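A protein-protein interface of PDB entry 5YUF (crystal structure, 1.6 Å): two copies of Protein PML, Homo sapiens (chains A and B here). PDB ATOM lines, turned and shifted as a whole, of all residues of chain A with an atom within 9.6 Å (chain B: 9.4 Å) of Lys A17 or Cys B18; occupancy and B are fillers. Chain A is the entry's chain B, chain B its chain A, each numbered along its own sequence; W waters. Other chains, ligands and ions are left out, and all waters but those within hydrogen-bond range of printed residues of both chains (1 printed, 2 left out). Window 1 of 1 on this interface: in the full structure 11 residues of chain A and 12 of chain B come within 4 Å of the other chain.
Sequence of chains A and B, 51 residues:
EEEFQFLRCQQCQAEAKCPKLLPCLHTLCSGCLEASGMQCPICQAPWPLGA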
ATOM      1  N   PHE A   4      29.470  -5.920  -8.606  1.00  0.00           N
ATOM      2  CA  PHE A   4      28.402  -5.612  -9.545  1.00  0.00           C
ATOM      3  C   PHE A   4      27.976  -4.156  -9.408  1.00  0.00           C
ATOM      4  O   PHE A   4      28.066  -3.560  -8.330  1.00  0.00           O
ATOM      5  CB  PHE A   4      27.179  -6.520  -9.361  1.00  0.00           C
ATOM      6  CG  PHE A   4      27.460  -7.975  -9.613  1.00  0.00           C
ATOM      7  CD1 PHE A   4      27.727  -8.423 -10.896  1.00  0.00           C
ATOM      8  CD2 PHE A   4      27.382  -8.902  -8.593  1.00  0.00           C
ATOM      9  CE1 PHE A   4      27.972  -9.758 -11.149  1.00  0.00           C
ATOM     10  CE2 PHE A   4      27.623 -10.247  -8.839  1.00  0.00           C
ATOM     11  CZ  PHE A   4      27.911 -10.673 -10.120  1.00  0.00           C
ATOM     12  N   GLN A   5      27.560  -3.582 -10.534  1.00  0.00           N
ATOM     13  CA  GLN A   5      27.049  -2.222 -10.607  1.00  0.00           C
ATOM     14  C   GLN A   5      25.524  -2.203 -10.599  1.00  0.00           C
ATOM     15  O   GLN A   5      24.849  -3.237 -10.581  1.00  0.00           O
ATOM     16  CB  GLN A   5      27.624  -1.510 -11.830  1.00  0.00           C
ATOM     17  CG  GLN A   5      29.117  -1.222 -11.688  1.00  0.00           C
ATOM     18  CD  GLN A   5      29.976  -2.429 -11.966  1.00  0.00           C
ATOM     19  OE1 GLN A   5      29.874  -3.059 -13.018  1.00  0.00           O
ATOM     20  NE2 GLN A   5      30.806  -2.784 -10.993  1.00  0.00           N
ATOM     21  N   PHE A   6      24.976  -0.994 -10.581  1.00  0.00           N
ATOM     22  CA  PHE A   6      23.537  -0.794 -10.558  1.00  0.00           C
ATOM     23  C   PHE A   6      22.940  -0.780 -11.962  1.00  0.00           C
ATOM     24  O   PHE A   6      23.640  -0.615 -12.967  1.00  0.00           O
ATOM     25  CB  PHE A   6      23.213   0.522  -9.846  1.00  0.00           C
ATOM     26  CG  PHE A   6      23.547   0.513  -8.381  1.00  0.00           C
ATOM     27  CD1 PHE A   6      22.777  -0.220  -7.488  1.00  0.00           C
ATOM     28  CD2 PHE A   6      24.619   1.244  -7.896  1.00  0.00           C
ATOM     29  CE1 PHE A   6      23.076  -0.231  -6.141  1.00  0.00           C
ATOM     30  CE2 PHE A   6      24.924   1.239  -6.548  1.00  0.00           C
ATOM     31  CZ  PHE A   6      24.152   0.504  -5.669  1.00  0.00           C
ATOM     32  N   LEU A   7      21.616  -0.917 -12.006  1.00  0.00           N
ATOM     33  CA  LEU A   7      20.855  -0.834 -13.242  1.00  0.00           C
ATOM     34  C   LEU A   7      20.967   0.562 -13.850  1.00  0.00           C
ATOM     35  O   LEU A   7      21.382   1.524 -13.198  1.00  0.00           O
ATOM     36  CB  LEU A   7      19.381  -1.161 -12.980  1.00  0.00           C
ATOM     37  CG  LEU A   7      19.083  -2.568 -12.465  1.00  0.00           C
ATOM     38  CD1 LEU A   7      17.659  -2.658 -11.948  1.00  0.00           C
ATOM     39  CD2 LEU A   7      19.296  -3.556 -13.590  1.00  0.00           C
ATOM     40  N   ARG A   8      20.617   0.653 -15.133  1.00  0.00           N
ATOM     41  CA  ARG A   8      20.631   1.911 -15.870  1.00  0.00           C
ATOM     42  C   ARG A   8      19.200   2.358 -16.159  1.00  0.00           C
ATOM     43  O   ARG A   8      18.332   1.531 -16.433  1.00  0.00           O
ATOM     44  CB  ARG A   8      21.391   1.764 -17.191  1.00  0.00           C
ATOM     45  CG  ARG A   8      22.814   1.213 -17.052  1.00  0.00           C
ATOM     46  CD  ARG A   8      23.694   1.988 -16.088  1.00  0.00           C
ATOM     47  NE  ARG A   8      24.080   3.301 -16.601  1.00  0.00           N
ATOM     48  CZ  ARG A   8      25.165   3.957 -16.205  1.00  0.00           C
ATOM     49  NH1 ARG A   8      25.961   3.436 -15.287  1.00  0.00           N
ATOM     50  NH2 ARG A   8      25.447   5.141 -16.720  1.00  0.00           N
ATOM     51  N   CYS A   9      18.955   3.666 -16.058  1.00  0.00           N
ATOM     52  CA  CYS A   9      17.686   4.255 -16.481  1.00  0.00           C
ATOM     53  C   CYS A   9      17.486   4.102 -17.986  1.00  0.00           C
ATOM     54  O   CYS A   9      18.356   4.466 -18.780  1.00  0.00           O
ATOM     55  CB  CYS A   9      17.659   5.736 -16.097  1.00  0.00           C
ATOM     56  SG  CYS A   9      16.150   6.617 -16.589  1.00  0.00           S
ATOM     57  N   ALA A  14      21.499   7.168 -17.288  1.00  0.00           N
ATOM     58  CA  ALA A  14      22.240   7.280 -16.043  1.00  0.00           C
ATOM     59  C   ALA A  14      21.970   6.062 -15.159  1.00  0.00           C
ATOM     60  O   ALA A  14      21.198   5.170 -15.506  1.00  0.00           O
ATOM     61  CB  ALA A  14      21.869   8.573 -15.321  1.00  0.00           C
ATOM     62  N   GLU A  15      22.640   6.011 -14.011  1.00  0.00           N
ATOM     63  CA  GLU A  15      22.360   4.974 -13.026  1.00  0.00           C
ATOM     64  C   GLU A  15      20.949   5.121 -12.486  1.00  0.00           C
ATOM     65  O   GLU A  15      20.483   6.234 -12.219  1.00  0.00           O
ATOM     66  CB  GLU A  15      23.317   5.068 -11.840  1.00  0.00           C
ATOM     67  CG  GLU A  15      24.731   4.651 -12.064  1.00  0.00           C
ATOM     68  CD  GLU A  15      25.575   4.960 -10.844  1.00  0.00           C
ATOM     69  OE1 GLU A  15      25.801   6.158 -10.577  1.00  0.00           O
ATOM     70  OE2 GLU A  15      25.975   4.012 -10.139  1.00  0.00           O
ATOM     71  N   ALA A  16      20.284   3.985 -12.288  1.00  0.00           N
ATOM     72  CA  ALA A  16      19.000   3.907 -11.596  1.00  0.00           C
ATOM     73  C   ALA A  16      19.232   2.957 -10.429  1.00  0.00           C
ATOM     74  O   ALA A  16      19.045   1.746 -10.562  1.00  0.00           O
ATOM     75  CB  ALA A  16      17.892   3.412 -12.510  1.00  0.00           C
ATOM     76  N   LYS A  17      19.646   3.503  -9.286  1.00  0.00           N
ATOM     77  CA  LYS A  17      20.146   2.653  -8.209  1.00  0.00           C
ATOM     78  C   LYS A  17      19.028   1.845  -7.562  1.00  0.00           C
ATOM     79  O   LYS A  17      19.169   0.636  -7.349  1.00  0.00           O
ATOM     80  CB  LYS A  17      20.870   3.502  -7.170  1.00  0.00           C
ATOM     81  CG  LYS A  17      22.188   4.044  -7.680  1.00  0.00           C
ATOM     82  CD  LYS A  17      22.860   4.928  -6.659  1.00  0.00           C
ATOM     83  CE  LYS A  17      24.333   5.082  -6.971  1.00  0.00           C
ATOM     84  NZ  LYS A  17      25.002   5.985  -5.999  1.00  0.00           N
ATOM     85  N   CYS A  18      17.910   2.487  -7.240  1.00  0.00           N
ATOM     86  CA  CYS A  18      16.805   1.831  -6.539  1.00  0.00           C
ATOM     87  C   CYS A  18      15.511   2.105  -7.302  1.00  0.00           C
ATOM     88  O   CYS A  18      14.669   2.899  -6.872  1.00  0.00           O
ATOM     89  CB  CYS A  18      16.731   2.320  -5.091  1.00  0.00           C
ATOM     90  SG  CYS A  18      18.364   2.421  -4.283  1.00  0.00           S
ATOM     91  N   PRO A  19      15.331   1.458  -8.451  1.00  0.00           N
ATOM     92  CA  PRO A  19      14.175   1.771  -9.300  1.00  0.00           C
ATOM     93  C   PRO A  19      12.876   1.234  -8.723  1.00  0.00           C
ATOM     94  O   PRO A  19      12.833   0.185  -8.076  1.00  0.00           O
ATOM     95  CB  PRO A  19      14.512   1.085 -10.630  1.00  0.00           C
ATOM     96  CG  PRO A  19      15.474  -0.001 -10.272  1.00  0.00           C
ATOM     97  CD  PRO A  19      16.229   0.466  -9.063  1.00  0.00           C
ATOM     98  N   LYS A  20      11.805   1.983  -8.962  1.00  0.00           N
ATOM     99  CA  LYS A  20      10.476   1.562  -8.555  1.00  0.00           C
ATOM    100  C   LYS A  20       9.885   0.578  -9.554  1.00  0.00           C
ATOM    101  O   LYS A  20      10.230   0.578 -10.740  1.00  0.00           O
ATOM    102  CB  LYS A  20       9.540   2.765  -8.433  1.00  0.00           C
ATOM    103  CG  LYS A  20       9.959   3.791  -7.406  1.00  0.00           C
ATOM    104  CD  LYS A  20       9.989   3.174  -6.023  1.00  0.00           C
ATOM    105  CE  LYS A  20      10.371   4.184  -4.971  1.00  0.00           C
ATOM    106  NZ  LYS A  20       9.947   3.713  -3.630  1.00  0.00           N
ATOM    107  N   THR A  27      12.653   0.570 -16.467  1.00  0.00           N
ATOM    108  CA  THR A  27      13.498   0.962 -15.350  1.00  0.00           C
ATOM    109  C   THR A  27      13.786   2.447 -15.488  1.00  0.00           C
ATOM    110  O   THR A  27      14.350   2.867 -16.503  1.00  0.00           O
ATOM    111  CB  THR A  27      14.796   0.159 -15.371  1.00  0.00           C
ATOM    112  OG1 THR A  27      14.497  -1.232 -15.245  1.00  0.00           O
ATOM    113  CG2 THR A  27      15.740   0.590 -14.252  1.00  0.00           C
ATOM    114  N   LEU A  28      13.422   3.232 -14.476  1.00  0.00           N
ATOM    115  CA  LEU A  28      13.650   4.673 -14.477  1.00  0.00           C
ATOM    116  C   LEU A  28      14.437   5.094 -13.243  1.00  0.00           C
ATOM    117  O   LEU A  28      14.222   4.562 -12.152  1.00  0.00           O
ATOM    118  CB  LEU A  28      12.332   5.442 -14.487  1.00  0.00           C
ATOM    119  CG  LEU A  28      11.416   5.198 -15.678  1.00  0.00           C
ATOM    120  CD1 LEU A  28      10.105   5.945 -15.473  1.00  0.00           C
ATOM    121  CD2 LEU A  28      12.080   5.640 -16.966  1.00  0.00           C
ATOM    122  N   CYS A  29      15.349   6.053 -13.412  1.00  0.00           N
ATOM    123  CA  CYS A  29      15.951   6.704 -12.254  1.00  0.00           C
ATOM    124  C   CYS A  29      14.915   7.587 -11.563  1.00  0.00           C
ATOM    125  O   CYS A  29      13.863   7.908 -12.121  1.00  0.00           O
ATOM    126  CB  CYS A  29      17.172   7.538 -12.652  1.00  0.00           C
ATOM    127  SG  CYS A  29      16.840   9.044 -13.607  1.00  0.00           S
ATOM    128  N   SER A  30      15.221   7.982 -10.324  1.00  0.00           N
ATOM    129  CA  SER A  30      14.245   8.738  -9.545  1.00  0.00           C
ATOM    130  C   SER A  30      13.942  10.081 -10.197  1.00  0.00           C
ATOM    131  O   SER A  30      12.799  10.551 -10.170  1.00  0.00           O
ATOM    132  CB  SER A  30      14.746   8.939  -8.118  1.00  0.00           C
ATOM    133  OG  SER A  30      15.974   9.627  -8.123  1.00  0.00           O
ATOM    134  N   GLY A  31      14.957  10.722 -10.778  1.00  0.00           N
ATOM    135  CA  GLY A  31      14.731  11.974 -11.479  1.00  0.00           C
ATOM    136  C   GLY A  31      13.739  11.836 -12.614  1.00  0.00           C
ATOM    137  O   GLY A  31      12.804  12.630 -12.742  1.00  0.00           O
ATOM    138  N   PHE B   6       9.050  -0.913  -4.372  1.00  0.00           N
ATOM    139  CA  PHE B   6      10.344  -1.356  -4.865  1.00  0.00           C
ATOM    140  C   PHE B   6      10.202  -2.742  -5.491  1.00  0.00           C
ATOM    141  O   PHE B   6       9.187  -3.424  -5.331  1.00  0.00           O
ATOM    142  CB  PHE B   6      11.394  -1.371  -3.749  1.00  0.00           C
ATOM    143  CG  PHE B   6      11.780  -0.002  -3.242  1.00  0.00           C
ATOM    144  CD1 PHE B   6      12.556   0.849  -4.017  1.00  0.00           C
ATOM    145  CD2 PHE B   6      11.403   0.417  -1.977  1.00  0.00           C
ATOM    146  CE1 PHE B   6      12.920   2.102  -3.551  1.00  0.00           C
ATOM    147  CE2 PHE B   6      11.767   1.666  -1.504  1.00  0.00           C
ATOM    148  CZ  PHE B   6      12.531   2.506  -2.289  1.00  0.00           C
ATOM    149  N   LEU B   7      11.235  -3.153  -6.221  1.00  0.00           N
ATOM    150  CA  LEU B   7      11.260  -4.471  -6.837  1.00  0.00           C
ATOM    151  C   LEU B   7      11.317  -5.585  -5.784  1.00  0.00           C
ATOM    152  O   LEU B   7      11.630  -5.363  -4.611  1.00  0.00           O
ATOM    153  CB  LEU B   7      12.445  -4.588  -7.795  1.00  0.00           C
ATOM    154  CG  LEU B   7      12.466  -3.593  -8.960  1.00  0.00           C
ATOM    155  CD1 LEU B   7      13.804  -3.663  -9.686  1.00  0.00           C
ATOM    156  CD2 LEU B   7      11.304  -3.806  -9.925  1.00  0.00           C
ATOM    157  N   ARG B   8      10.982  -6.798  -6.228  1.00  0.00           N
ATOM    158  CA  ARG B   8      10.990  -8.008  -5.412  1.00  0.00           C
ATOM    159  C   ARG B   8      12.131  -8.938  -5.816  1.00  0.00           C
ATOM    160  O   ARG B   8      12.400  -9.129  -7.007  1.00  0.00           O
ATOM    161  CB  ARG B   8       9.658  -8.750  -5.561  1.00  0.00           C
ATOM    162  CG  ARG B   8       8.430  -7.974  -5.085  1.00  0.00           C
ATOM    163  CD  ARG B   8       8.060  -8.266  -3.629  1.00  0.00           C
ATOM    164  NE  ARG B   8       8.293  -7.159  -2.711  1.00  0.00           N
ATOM    165  CZ  ARG B   8       8.231  -7.272  -1.387  1.00  0.00           C
ATOM    166  NH1 ARG B   8       7.897  -8.430  -0.831  1.00  0.00           N
ATOM    167  NH2 ARG B   8       8.465  -6.222  -0.615  1.00  0.00           N
ATOM    168  N   CYS B   9      12.783  -9.536  -4.819  1.00  0.00           N
ATOM    169  CA  CYS B   9      13.782 -10.568  -5.075  1.00  0.00           C
ATOM    170  C   CYS B   9      13.146 -11.796  -5.712  1.00  0.00           C
ATOM    171  O   CYS B   9      12.157 -12.327  -5.205  1.00  0.00           O
ATOM    172  CB  CYS B   9      14.474 -10.968  -3.774  1.00  0.00           C
ATOM    173  SG  CYS B   9      15.714 -12.265  -3.985  1.00  0.00           S
ATOM    174  N   ALA B  14      11.379 -11.395  -1.044  1.00  0.00           N
ATOM    175  CA  ALA B  14      11.424 -10.203  -0.210  1.00  0.00           C
ATOM    176  C   ALA B  14      11.630  -8.968  -1.090  1.00  0.00           C
ATOM    177  O   ALA B  14      11.825  -9.060  -2.304  1.00  0.00           O
ATOM    178  CB  ALA B  14      12.532 -10.313   0.831  1.00  0.00           C
ATOM    179  N   GLU B  15      11.585  -7.792  -0.467  1.00  0.00           N
ATOM    180  CA  GLU B  15      11.877  -6.560  -1.192  1.00  0.00           C
ATOM    181  C   GLU B  15      13.335  -6.550  -1.628  1.00  0.00           C
ATOM    182  O   GLU B  15      14.225  -6.972  -0.884  1.00  0.00           O
ATOM    183  CB  GLU B  15      11.597  -5.335  -0.319  1.00  0.00           C
ATOM    184  CG  GLU B  15      11.463  -4.035  -1.109  1.00  0.00           C
ATOM    185  CD  GLU B  15      11.096  -2.845  -0.238  1.00  0.00           C
ATOM    186  OE1 GLU B  15      10.157  -2.106  -0.609  1.00  0.00           O
ATOM    187  OE2 GLU B  15      11.656  -2.719   0.872  1.00  0.00           O
ATOM    188  N   ALA B  16      13.578  -6.073  -2.846  1.00  0.00           N
ATOM    189  CA  ALA B  16      14.926  -5.837  -3.362  1.00  0.00           C
ATOM    190  C   ALA B  16      14.975  -4.362  -3.758  1.00  0.00           C
ATOM    191  O   ALA B  16      14.619  -3.990  -4.876  1.00  0.00           O
ATOM    192  CB  ALA B  16      15.256  -6.762  -4.531  1.00  0.00           C
ATOM    193  N   LYS B  17      15.424  -3.528  -2.821  1.00  0.00           N
ATOM    194  CA  LYS B  17      15.288  -2.085  -2.972  1.00  0.00           C
ATOM    195  C   LYS B  17      16.243  -1.541  -4.029  1.00  0.00           C
ATOM    196  O   LYS B  17      15.844  -0.744  -4.882  1.00  0.00           O
ATOM    197  CB  LYS B  17      15.530  -1.417  -1.617  1.00  0.00           C
ATOM    198  CG  LYS B  17      15.247   0.068  -1.566  1.00  0.00           C
ATOM    199  CD  LYS B  17      15.879   0.674  -0.321  1.00  0.00           C
ATOM    200  CE  LYS B  17      15.708   2.180  -0.265  1.00  0.00           C
ATOM    201  NZ  LYS B  17      16.449   2.858  -1.358  1.00  0.00           N
ATOM    202  N   CYS B  18      17.510  -1.951  -3.991  1.00  0.00           N
ATOM    203  CA  CYS B  18      18.519  -1.458  -4.931  1.00  0.00           C
ATOM    204  C   CYS B  18      19.267  -2.644  -5.522  1.00  0.00           C
ATOM    205  O   CYS B  18      20.437  -2.895  -5.196  1.00  0.00           O
ATOM    206  CB  CYS B  18      19.463  -0.476  -4.237  1.00  0.00           C
ATOM    207  SG  CYS B  18      18.598   0.722  -3.176  1.00  0.00           S
ATOM    208  N   PRO B  19      18.627  -3.399  -6.413  1.00  0.00           N
ATOM    209  CA  PRO B  19      19.247  -4.622  -6.926  1.00  0.00           C
ATOM    210  C   PRO B  19      20.388  -4.327  -7.888  1.00  0.00           C
ATOM    211  O   PRO B  19      20.326  -3.389  -8.686  1.00  0.00           O
ATOM    212  CB  PRO B  19      18.096  -5.341  -7.637  1.00  0.00           C
ATOM    213  CG  PRO B  19      17.125  -4.272  -7.973  1.00  0.00           C
ATOM    214  CD  PRO B  19      17.258  -3.206  -6.929  1.00  0.00           C
ATOM    215  N   LYS B  20      21.414  -5.172  -7.829  1.00  0.00           N
ATOM    216  CA  LYS B  20      22.553  -5.086  -8.728  1.00  0.00           C
ATOM    217  C   LYS B  20      22.248  -5.718 -10.080  1.00  0.00           C
ATOM    218  O   LYS B  20      21.383  -6.594 -10.214  1.00  0.00           O
ATOM    219  CB  LYS B  20      23.772  -5.778  -8.111  1.00  0.00           C
ATOM    220  CG  LYS B  20      24.330  -5.142  -6.850  1.00  0.00           C
ATOM    221  CD  LYS B  20      24.887  -3.764  -7.165  1.00  0.00           C
ATOM    222  CE  LYS B  20      25.537  -3.109  -5.970  1.00  0.00           C
ATOM    223  NZ  LYS B  20      26.482  -2.056  -6.437  1.00  0.00           N
ATOM    224  N   LEU B  21      22.952  -5.234 -11.096  1.00  0.00           N
ATOM    225  CA  LEU B  21      22.891  -5.800 -12.438  1.00  0.00           C
ATOM    226  C   LEU B  21      23.756  -7.051 -12.502  1.00  0.00           C
ATOM    227  O   LEU B  21      24.985  -6.972 -12.372  1.00  0.00           O
ATOM    228  CB  LEU B  21      23.352  -4.760 -13.453  1.00  0.00           C
ATOM    229  CG  LEU B  21      23.362  -5.176 -14.921  1.00  0.00           C
ATOM    230  CD1 LEU B  21      21.976  -5.597 -15.377  1.00  0.00           C
ATOM    231  CD2 LEU B  21      23.881  -4.013 -15.750  1.00  0.00           C
ATOM    232  N   LEU B  22      23.116  -8.198 -12.726  1.00  0.00           N
ATOM    233  CA  LEU B  22      23.770  -9.487 -12.806  1.00  0.00           C
ATOM    234  C   LEU B  22      23.930  -9.923 -14.253  1.00  0.00           C
ATOM    235  O   LEU B  22      23.242  -9.426 -15.149  1.00  0.00           O
ATOM    236  CB  LEU B  22      22.944 -10.523 -12.045  1.00  0.00           C
ATOM    237  CG  LEU B  22      22.532 -10.089 -10.642  1.00  0.00           C
ATOM    238  CD1 LEU B  22      21.697 -11.175  -9.987  1.00  0.00           C
ATOM    239  CD2 LEU B  22      23.756  -9.750  -9.784  1.00  0.00           C
ATOM    240  N   THR B  27      16.807 -10.616 -10.674  1.00  0.00           N
ATOM    241  CA  THR B  27      16.743  -9.592  -9.634  1.00  0.00           C
ATOM    242  C   THR B  27      16.901 -10.269  -8.278  1.00  0.00           C
ATOM    243  O   THR B  27      16.121 -11.159  -7.939  1.00  0.00           O
ATOM    244  CB  THR B  27      15.408  -8.842  -9.692  1.00  0.00           C
ATOM    245  OG1 THR B  27      15.258  -8.203 -10.961  1.00  0.00           O
ATOM    246  CG2 THR B  27      15.335  -7.777  -8.608  1.00  0.00           C
ATOM    247  N   LEU B  28      17.911  -9.854  -7.505  1.00  0.00           N
ATOM    248  CA  LEU B  28      18.168 -10.426  -6.188  1.00  0.00           C
ATOM    249  C   LEU B  28      18.232  -9.329  -5.135  1.00  0.00           C
ATOM    250  O   LEU B  28      18.737  -8.237  -5.404  1.00  0.00           O
ATOM    251  CB  LEU B  28      19.479 -11.204  -6.168  1.00  0.00           C
ATOM    252  CG  LEU B  28      19.607 -12.379  -7.130  1.00  0.00           C
ATOM    253  CD1 LEU B  28      20.986 -13.009  -7.035  1.00  0.00           C
ATOM    254  CD2 LEU B  28      18.516 -13.402  -6.859  1.00  0.00           C
ATOM    255  N   CYS B  29      17.718  -9.620  -3.940  1.00  0.00           N
ATOM    256  CA  CYS B  29      17.965  -8.758  -2.792  1.00  0.00           C
ATOM    257  C   CYS B  29      19.427  -8.874  -2.363  1.00  0.00           C
ATOM    258  O   CYS B  29      20.165  -9.761  -2.796  1.00  0.00           O
ATOM    259  CB  CYS B  29      17.037  -9.109  -1.626  1.00  0.00           C
ATOM    260  SG  CYS B  29      17.373 -10.695  -0.815  1.00  0.00           S
ATOM    261  N   SER B  30      19.861  -7.935  -1.524  1.00  0.00           N
ATOM    262  CA  SER B  30      21.268  -7.903  -1.135  1.00  0.00           C
ATOM    263  C   SER B  30      21.661  -9.146  -0.346  1.00  0.00           C
ATOM    264  O   SER B  30      22.762  -9.674  -0.527  1.00  0.00           O
ATOM    265  CB  SER B  30      21.559  -6.645  -0.320  1.00  0.00           C
ATOM    266  OG  SER B  30      20.747  -6.586   0.836  1.00  0.00           O
ATOM    267  N   GLY B  31      20.774  -9.627   0.527  1.00  0.00           N
ATOM    268  CA  GLY B  31      21.053 -10.848   1.272  1.00  0.00           C
ATOM    269  C   GLY B  31      21.285 -12.047   0.374  1.00  0.00           C
ATOM    270  O   GLY B  31      22.252 -12.794   0.549  1.00  0.00           O
ATOM    271  N   LEU B  33      22.120 -12.026  -2.749  1.00  0.00           N
ATOM    272  CA  LEU B  33      23.347 -11.854  -3.518  1.00  0.00           C
ATOM    273  C   LEU B  33      24.564 -12.178  -2.655  1.00  0.00           C
ATOM    274  O   LEU B  33      25.495 -12.862  -3.098  1.00  0.00           O
ATOM    275  CB  LEU B  33      23.414 -10.430  -4.081  1.00  0.00           C
ATOM    276  CG  LEU B  33      24.577 -10.136  -5.030  1.00  0.00           C
ATOM    277  CD1 LEU B  33      24.573 -11.088  -6.209  1.00  0.00           C
ATOM    278  CD2 LEU B  33      24.510  -8.707  -5.520  1.00  0.00           C
HETATM  279  O   HOH W   1      26.989  -5.191 -13.056  1.00  0.00           O
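O of Gln A5 lies within hydrogen-bond range of N of Leu B21 (2.8 Å). The side-chain sulfur (SG) of Cys A18 forms a disulfide with the side-chain sulfur (SG) of Cys B18. The backbone carbonyl oxygen (O) of Phe A4 is in hydrogen-bond range of the side-chain amino group (NZ) of Lys B20 (2.9 Å). The side-chain amino group (NZ) of Lys B17 sits at hydrogen-bond distance from the side-chain sulfur (SG) of Cys A18.
O of Leu B7 is in hydrogen-bond range of N of Ala B16. The backbone NH (N) of Ala A16 is in hydrogen-bond range of the backbone carbonyl oxygen (O) of Leu A7 (2.8 Å). NZ of Lys B17 lies close to SG of Cys B18, 3.5 Å away.
Among the printed residues, pairs that only touch across the chains: Phe A4 with Leu B21, Phe A4 with Leu B22, Gln A5 with Lys B20, Phe A6 with Cys B18, Phe A6 with Lys B20, Leu A7 with Leu B21, Lys A17 with Cys B18, Cys A18 with Phe B6, Pro A19 with Leu B7 and Lys A20 with Phe B6.
Of chain B, only Cys B18 (3.3 Å) comes within 4 Å of Lys A17. Printed residues of chain A within 4 Å of Cys B18: Phe A6, Lys A17 and Cys A18. No residue of chain B comes within 4 Å of Ala A16. No residue of chain A comes within 4 Å of Pro B19. Printed residues of chain B within 4 Å of Lys A20: Phe B6. Of the printed residues of chain A, Leu B7 touches Pro A19 (3.9 Å). Of the printed residues of chain B, Phe A4 touches Lys B20 (2.9 Å), Leu B21 (3.4 Å) and Leu B22 (3.9 Å). Leu A28 touches none of the printed residues of chain B. Arg A8 touches none of the printed residues of chain B. The nearest residue of chain B that does not touch Lys A17 is Pro B19 (4.2 Å). The nearest residue of chain A that does not touch Cys B18 is Pro A19 (5.1 Å). The nearest printed residue of chain A that does not touch Leu B22 is Gln A5 (5.7 Å).
Printed residues of chain A that touch a printed residue of chain B: Phe A4, Gln A5, Phe A6, Leu A7, Lys A17, Cys A18, Pro A19 and Lys A20. Among the printed residues, 14 pairs touch across the chains.
Phe A6 touches Cys B18, and with the chains exchanged Cys A18 touches Phe B6. Phe A6 touches Lys B20, and with the chains exchanged Lys A20 touches Phe B6. Lys A17 touches Cys B18, and with the chains exchanged Cys A18 touches Lys B17. Pro A19 touches Leu B7, but with the chains exchanged Leu A7 does not touch Pro B19 (4.1 Å). Of the 14 pairs that touch across the chains among the printed residues, 7 have their exchanged pair printed and touching as well.
Water W1 bridges the backbone carbonyl oxygen of Leu B21 (2.8 Å) and the backbone NH of Gln A5 (3.0 Å).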
